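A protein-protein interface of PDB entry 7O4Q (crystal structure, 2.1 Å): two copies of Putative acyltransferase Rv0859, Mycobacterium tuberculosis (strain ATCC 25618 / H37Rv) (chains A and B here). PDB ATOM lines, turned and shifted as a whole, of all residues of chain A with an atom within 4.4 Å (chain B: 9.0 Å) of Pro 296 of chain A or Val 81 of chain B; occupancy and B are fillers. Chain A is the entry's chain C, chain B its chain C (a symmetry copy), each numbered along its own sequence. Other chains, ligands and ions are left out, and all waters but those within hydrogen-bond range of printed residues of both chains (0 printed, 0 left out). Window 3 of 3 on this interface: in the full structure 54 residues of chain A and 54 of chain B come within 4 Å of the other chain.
Val 81 of chain B touches Gly 293 of chain A (O to CA, 3.5 Å).
Thr 82 of chain B touches Gly 293 of chain A (CG2 to O, 3.3 Å).
O of Ala 294 of chain A touches CB of Val 81 of chain B, at 3.2 Å.
Pro 296 of chain A touches Leu 75 of chain B.
Pro 296 of chain A touches Val 81 of chain B (CD to CG1, 3.7 Å).
NH2 of Arg 71 of chain B touches C of Gly 393 of chain A (3.9 Å).
Pro 296 of chain A touches just these residues of chain B: Leu 75 (3.8 Å) and Val 81 (3.7 Å).
Printed residues of chain A within 4 Å of Val 81 of chain B: Gly 293, Ala 294 and Pro 296.
No residue of chain B comes within 4 Å of Val 297 of chain A.
Printed residues of chain B within 4 Å of Gly 392 of chain A: Arg 71.
Of the printed residues of chain B, Gly 393 of chain A touches Arg 71 (3.9 Å).
Of the printed residues of chain A, Arg 71 of chain B touches Gly 392 and Gly 393.
Pro 80 of chain B touches none of the printed residues of chain A.
The nearest printed residue of chain A that does not touch Leu 75 of chain B is Gly 392 of chain A (4.01 Å).
The guanidinium group (NH2) of Arg 71 of chain B sits at hydrogen-bond distance from the backbone carbonyl oxygen (O) of Gly 392 of chain A (2.6 Å).
The guanidinium group (NH1) of Arg 71 of chain B is in hydrogen-bond range of the backbone carbonyl oxygen (O) of Gly 84 of chain B, 2.8 Å away.
The backbone NH (N) of Ala 294 of chain A lies within hydrogen-bond range of the backbone carbonyl oxygen (O) of Gly 393 of chain A (2.6 Å).
The backbone carbonyl oxygen (O) of Val 81 of chain B lies within hydrogen-bond range of the guanidinium group (NH2) of Arg 71 of chain B (2.9 Å).
Hydrophobic or aromatic side chains of chain A within 4 Å of the printed part of chain B: Pro 296.
Hydrophobic or aromatic side chains of chain B that line the printed part of chain A: Leu 75 and Val 81.
No position is printed for both chains.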
ATOM      1  N   GLY A 293     -11.021   3.953  15.831  1.00  0.00           N
ATOM      2  CA  GLY A 293     -11.722   4.162  14.579  1.00  0.00           C
ATOM      3  C   GLY A 293     -10.901   3.657  13.412  1.00  0.00           C
ATOM      4  O   GLY A 293      -9.726   3.302  13.549  1.00  0.00           O
ATOM      5  N   ALA A 294     -11.551   3.630  12.251  1.00  0.00           N
ATOM      6  CA  ALA A 294     -10.929   3.212  11.003  1.00  0.00           C
ATOM      7  C   ALA A 294     -11.412   4.150   9.902  1.00  0.00           C
ATOM      8  O   ALA A 294     -12.006   5.199  10.175  1.00  0.00           O
ATOM      9  CB  ALA A 294     -11.243   1.740  10.703  1.00  0.00           C
ATOM     10  N   ASP A 295     -11.164   3.761   8.653  1.00  0.00           N
ATOM     11  CA  ASP A 295     -11.487   4.605   7.509  1.00  0.00           C
ATOM     12  C   ASP A 295     -12.967   4.988   7.508  1.00  0.00           C
ATOM     13  O   ASP A 295     -13.832   4.111   7.654  1.00  0.00           O
ATOM     14  CB  ASP A 295     -11.131   3.882   6.212  1.00  0.00           C
ATOM     15  CG  ASP A 295     -11.767   4.521   4.997  1.00  0.00           C
ATOM     16  OD1 ASP A 295     -11.484   5.708   4.733  1.00  0.00           O
ATOM     17  OD2 ASP A 295     -12.548   3.834   4.306  1.00  0.00           O
ATOM     18  N   PRO A 296     -13.301   6.275   7.347  1.00  0.00           N
ATOM     19  CA  PRO A 296     -14.719   6.672   7.352  1.00  0.00           C
ATOM     20  C   PRO A 296     -15.470   6.339   6.071  1.00  0.00           C
ATOM     21  O   PRO A 296     -16.709   6.348   6.088  1.00  0.00           O
ATOM     22  CB  PRO A 296     -14.653   8.190   7.567  1.00  0.00           C
ATOM     23  CG  PRO A 296     -13.334   8.585   6.982  1.00  0.00           C
ATOM     24  CD  PRO A 296     -12.398   7.436   7.261  1.00  0.00           C
ATOM     25  N   VAL A 297     -14.774   6.052   4.967  1.00  0.00           N
ATOM     26  CA  VAL A 297     -15.463   5.723   3.722  1.00  0.00           C
ATOM     27  C   VAL A 297     -16.093   4.340   3.812  1.00  0.00           C
ATOM     28  O   VAL A 297     -17.279   4.159   3.508  1.00  0.00           O
ATOM     29  CB  VAL A 297     -14.500   5.833   2.527  1.00  0.00           C
ATOM     30  CG1 VAL A 297     -15.160   5.305   1.258  1.00  0.00           C
ATOM     31  CG2 VAL A 297     -14.053   7.279   2.343  1.00  0.00           C
ATOM     32  N   ILE A 298     -15.311   3.340   4.229  1.00  0.00           N
ATOM     33  CA  ILE A 298     -15.886   2.025   4.494  1.00  0.00           C
ATOM     34  C   ILE A 298     -16.704   2.058   5.781  1.00  0.00           C
ATOM     35  O   ILE A 298     -17.622   1.247   5.965  1.00  0.00           O
ATOM     36  CB  ILE A 298     -14.775   0.956   4.534  1.00  0.00           C
ATOM     37  CG1 ILE A 298     -15.348  -0.428   4.224  1.00  0.00           C
ATOM     38  CG2 ILE A 298     -14.066   0.949   5.884  1.00  0.00           C
ATOM     39  CD1 ILE A 298     -14.280  -1.477   4.003  1.00  0.00           C
ATOM     40  N   MET A 299     -16.371   2.975   6.695  1.00  0.00           N
ATOM     41  CA  MET A 299     -17.209   3.383   7.822  1.00  0.00           C
ATOM     42  C   MET A 299     -17.395   2.324   8.904  1.00  0.00           C
ATOM     43  O   MET A 299     -17.337   2.643  10.096  1.00  0.00           O
ATOM     44  CB  MET A 299     -18.582   3.836   7.314  1.00  0.00           C
ATOM     45  CG  MET A 299     -19.477   4.421   8.393  1.00  0.00           C
ATOM     46  SD  MET A 299     -21.005   5.121   7.736  1.00  0.00           S
ATOM     47  CE  MET A 299     -20.353   6.414   6.682  1.00  0.00           C
ATOM     48  N   GLY A 392     -18.969   7.520  10.358  1.00  0.00           N
ATOM     49  CA  GLY A 392     -17.702   8.213  10.335  1.00  0.00           C
ATOM     50  C   GLY A 392     -16.494   7.346  10.622  1.00  0.00           C
ATOM     51  O   GLY A 392     -15.385   7.882  10.754  1.00  0.00           O
ATOM     52  N   GLY A 393     -16.672   6.029  10.735  1.00  0.00           N
ATOM     53  CA  GLY A 393     -15.560   5.127  10.940  1.00  0.00           C
ATOM     54  C   GLY A 393     -15.125   4.936  12.374  1.00  0.00           C
ATOM     55  O   GLY A 393     -14.087   4.307  12.606  1.00  0.00           O
ATOM     56  N   GLU B  48      -0.778  13.099  16.904  1.00  0.00           N
ATOM     57  CA  GLU B  48      -2.228  13.175  17.010  1.00  0.00           C
ATOM     58  C   GLU B  48      -2.884  11.812  17.188  1.00  0.00           C
ATOM     59  O   GLU B  48      -4.062  11.756  17.558  1.00  0.00           O
ATOM     60  CB  GLU B  48      -2.800  13.879  15.780  1.00  0.00           C
ATOM     61  CG  GLU B  48      -2.258  15.285  15.568  1.00  0.00           C
ATOM     62  CD  GLU B  48      -2.924  16.005  14.408  1.00  0.00           C
ATOM     63  OE1 GLU B  48      -3.950  15.501  13.902  1.00  0.00           O
ATOM     64  OE2 GLU B  48      -2.421  17.074  14.004  1.00  0.00           O
ATOM     65  N   ASN B  49      -2.158  10.718  16.940  1.00  0.00           N
ATOM     66  CA  ASN B  49      -2.716   9.393  17.181  1.00  0.00           C
ATOM     67  C   ASN B  49      -2.949   9.128  18.662  1.00  0.00           C
ATOM     68  O   ASN B  49      -3.687   8.199  19.001  1.00  0.00           O
ATOM     69  CB  ASN B  49      -1.801   8.317  16.600  1.00  0.00           C
ATOM     70  CG  ASN B  49      -1.599   8.471  15.109  1.00  0.00           C
ATOM     71  OD1 ASN B  49      -2.509   8.216  14.321  1.00  0.00           O
ATOM     72  ND2 ASN B  49      -0.401   8.886  14.714  1.00  0.00           N
ATOM     73  N   ILE B  51      -4.465  11.294  20.569  1.00  0.00           N
ATOM     74  CA  ILE B  51      -5.753  11.903  20.883  1.00  0.00           C
ATOM     75  C   ILE B  51      -6.840  10.861  20.649  1.00  0.00           C
ATOM     76  O   ILE B  51      -7.023  10.384  19.525  1.00  0.00           O
ATOM     77  CB  ILE B  51      -5.999  13.157  20.035  1.00  0.00           C
ATOM     78  CG1 ILE B  51      -4.891  14.186  20.274  1.00  0.00           C
ATOM     79  CG2 ILE B  51      -7.370  13.747  20.348  1.00  0.00           C
ATOM     80  CD1 ILE B  51      -5.100  15.491  19.532  1.00  0.00           C
ATOM     81  N   SER B  52      -7.558  10.502  21.711  1.00  0.00           N
ATOM     82  CA  SER B  52      -8.543   9.433  21.632  1.00  0.00           C
ATOM     83  C   SER B  52      -9.974   9.928  21.475  1.00  0.00           C
ATOM     84  O   SER B  52     -10.850   9.123  21.140  1.00  0.00           O
ATOM     85  CB  SER B  52      -8.454   8.531  22.870  1.00  0.00           C
ATOM     86  OG  SER B  52      -8.614   9.278  24.063  1.00  0.00           O
ATOM     87  N   ASP B  53     -10.243  11.213  21.701  1.00  0.00           N
ATOM     88  CA  ASP B  53     -11.610  11.695  21.572  1.00  0.00           C
ATOM     89  C   ASP B  53     -11.615  13.202  21.367  1.00  0.00           C
ATOM     90  O   ASP B  53     -10.680  13.909  21.752  1.00  0.00           O
ATOM     91  CB  ASP B  53     -12.457  11.330  22.799  1.00  0.00           C
ATOM     92  CG  ASP B  53     -13.883  10.947  22.432  1.00  0.00           C
ATOM     93  OD1 ASP B  53     -14.331  11.285  21.313  1.00  0.00           O
ATOM     94  OD2 ASP B  53     -14.554  10.303  23.264  1.00  0.00           O
ATOM     95  N   ARG B  71     -17.330  14.749  15.227  1.00  0.00           N
ATOM     96  CA  ARG B  71     -16.716  13.808  14.297  1.00  0.00           C
ATOM     97  C   ARG B  71     -16.452  14.464  12.948  1.00  0.00           C
ATOM     98  O   ARG B  71     -15.436  14.184  12.304  1.00  0.00           O
ATOM     99  CB  ARG B  71     -17.597  12.569  14.125  1.00  0.00           C
ATOM    100  CG  ARG B  71     -16.997  11.524  13.189  1.00  0.00           C
ATOM    101  CD  ARG B  71     -15.586  11.153  13.626  1.00  0.00           C
ATOM    102  NE  ARG B  71     -15.039  10.019  12.885  1.00  0.00           N
ATOM    103  CZ  ARG B  71     -13.871   9.448  13.160  1.00  0.00           C
ATOM    104  NH1 ARG B  71     -13.133   9.904  14.163  1.00  0.00           N
ATOM    105  NH2 ARG B  71     -13.440   8.421  12.439  1.00  0.00           N
ATOM    106  N   VAL B  74     -13.180  16.295  13.327  1.00  0.00           N
ATOM    107  CA  VAL B  74     -12.033  15.388  13.282  1.00  0.00           C
ATOM    108  C   VAL B  74     -11.685  15.038  11.844  1.00  0.00           C
ATOM    109  O   VAL B  74     -10.512  15.054  11.450  1.00  0.00           O
ATOM    110  CB  VAL B  74     -12.321  14.124  14.112  1.00  0.00           C
ATOM    111  CG1 VAL B  74     -11.220  13.091  13.919  1.00  0.00           C
ATOM    112  CG2 VAL B  74     -12.485  14.477  15.586  1.00  0.00           C
ATOM    113  N   LEU B  75     -12.696  14.724  11.031  1.00  0.00           N
ATOM    114  CA  LEU B  75     -12.436  14.303   9.659  1.00  0.00           C
ATOM    115  C   LEU B  75     -12.079  15.484   8.762  1.00  0.00           C
ATOM    116  O   LEU B  75     -11.176  15.376   7.926  1.00  0.00           O
ATOM    117  CB  LEU B  75     -13.647  13.549   9.106  1.00  0.00           C
ATOM    118  CG  LEU B  75     -13.957  12.229   9.816  1.00  0.00           C
ATOM    119  CD1 LEU B  75     -15.256  11.617   9.311  1.00  0.00           C
ATOM    120  CD2 LEU B  75     -12.803  11.250   9.654  1.00  0.00           C
ATOM    121  N   ALA B  76     -12.769  16.615   8.921  1.00  0.00           N
ATOM    122  CA  ALA B  76     -12.475  17.778   8.086  1.00  0.00           C
ATOM    123  C   ALA B  76     -11.093  18.348   8.376  1.00  0.00           C
ATOM    124  O   ALA B  76     -10.430  18.854   7.462  1.00  0.00           O
ATOM    125  CB  ALA B  76     -13.539  18.857   8.287  1.00  0.00           C
ATOM    126  N   GLY B  78      -8.442  16.696   9.169  1.00  0.00           N
ATOM    127  CA  GLY B  78      -7.351  15.782   8.896  1.00  0.00           C
ATOM    128  C   GLY B  78      -6.773  15.107  10.119  1.00  0.00           C
ATOM    129  O   GLY B  78      -5.681  14.536  10.040  1.00  0.00           O
ATOM    130  N   MET B  79      -7.466  15.166  11.253  1.00  0.00           N
ATOM    131  CA  MET B  79      -7.059  14.413  12.424  1.00  0.00           C
ATOM    132  C   MET B  79      -7.198  12.917  12.153  1.00  0.00           C
ATOM    133  O   MET B  79      -7.942  12.507  11.259  1.00  0.00           O
ATOM    134  CB  MET B  79      -7.900  14.822  13.632  1.00  0.00           C
ATOM    135  CG  MET B  79      -7.488  16.146  14.255  1.00  0.00           C
ATOM    136  SD  MET B  79      -8.490  16.567  15.695  1.00  0.00           S
ATOM    137  CE  MET B  79      -8.126  15.190  16.785  1.00  0.00           C
ATOM    138  N   PRO B  80      -6.478  12.079  12.901  1.00  0.00           N
ATOM    139  CA  PRO B  80      -6.554  10.634  12.659  1.00  0.00           C
ATOM    140  C   PRO B  80      -7.966  10.104  12.868  1.00  0.00           C
ATOM    141  O   PRO B  80      -8.724  10.603  13.702  1.00  0.00           O
ATOM    142  CB  PRO B  80      -5.579  10.048  13.686  1.00  0.00           C
ATOM    143  CG  PRO B  80      -4.655  11.170  14.020  1.00  0.00           C
ATOM    144  CD  PRO B  80      -5.496  12.408  13.948  1.00  0.00           C
ATOM    145  N   VAL B  81      -8.313   9.071  12.096  1.00  0.00           N
ATOM    146  CA  VAL B  81      -9.643   8.476  12.184  1.00  0.00           C
ATOM    147  C   VAL B  81      -9.897   7.797  13.517  1.00  0.00           C
ATOM    148  O   VAL B  81     -11.050   7.475  13.830  1.00  0.00           O
ATOM    149  CB  VAL B  81      -9.856   7.467  11.039  1.00  0.00           C
ATOM    150  CG1 VAL B  81      -9.670   8.152   9.696  1.00  0.00           C
ATOM    151  CG2 VAL B  81      -8.904   6.285  11.184  1.00  0.00           C
ATOM    152  N   THR B  82      -8.856   7.573  14.312  1.00  0.00           N
ATOM    153  CA  THR B  82      -8.991   6.996  15.643  1.00  0.00           C
ATOM    154  C   THR B  82      -9.295   8.033  16.716  1.00  0.00           C
ATOM    155  O   THR B  82      -9.347   7.678  17.898  1.00  0.00           O
ATOM    156  CB  THR B  82      -7.709   6.250  16.019  1.00  0.00           C
ATOM    157  OG1 THR B  82      -6.603   7.161  15.964  1.00  0.00           O
ATOM    158  CG2 THR B  82      -7.462   5.099  15.063  1.00  0.00           C
ATOM    159  N   SER B  83      -9.496   9.297  16.343  1.00  0.00           N
ATOM    160  CA  SER B  83      -9.619  10.387  17.302  1.00  0.00           C
ATOM    161  C   SER B  83     -11.048  10.623  17.774  1.00  0.00           C
ATOM    162  O   SER B  83     -11.300  11.628  18.447  1.00  0.00           O
ATOM    163  CB  SER B  83      -9.062  11.680  16.708  1.00  0.00           C
ATOM    164  OG  SER B  83      -7.659  11.594  16.549  1.00  0.00           O
ATOM    165  N   GLY B  84     -11.985   9.745  17.427  1.00  0.00           N
ATOM    166  CA  GLY B  84     -13.314   9.838  18.013  1.00  0.00           C
ATOM    167  C   GLY B  84     -14.097  11.040  17.515  1.00  0.00           C
ATOM    168  O   GLY B  84     -14.004  11.442  16.350  1.00  0.00           O
ATOM    169  N   GLY B  85     -14.888  11.620  18.417  1.00  0.00           N
ATOM    170  CA  GLY B  85     -15.818  12.679  18.074  1.00  0.00           C
ATOM    171  C   GLY B  85     -17.212  12.422  18.617  1.00  0.00           C
ATOM    172  O   GLY B  85     -17.899  11.501  18.163  1.00  0.00           O
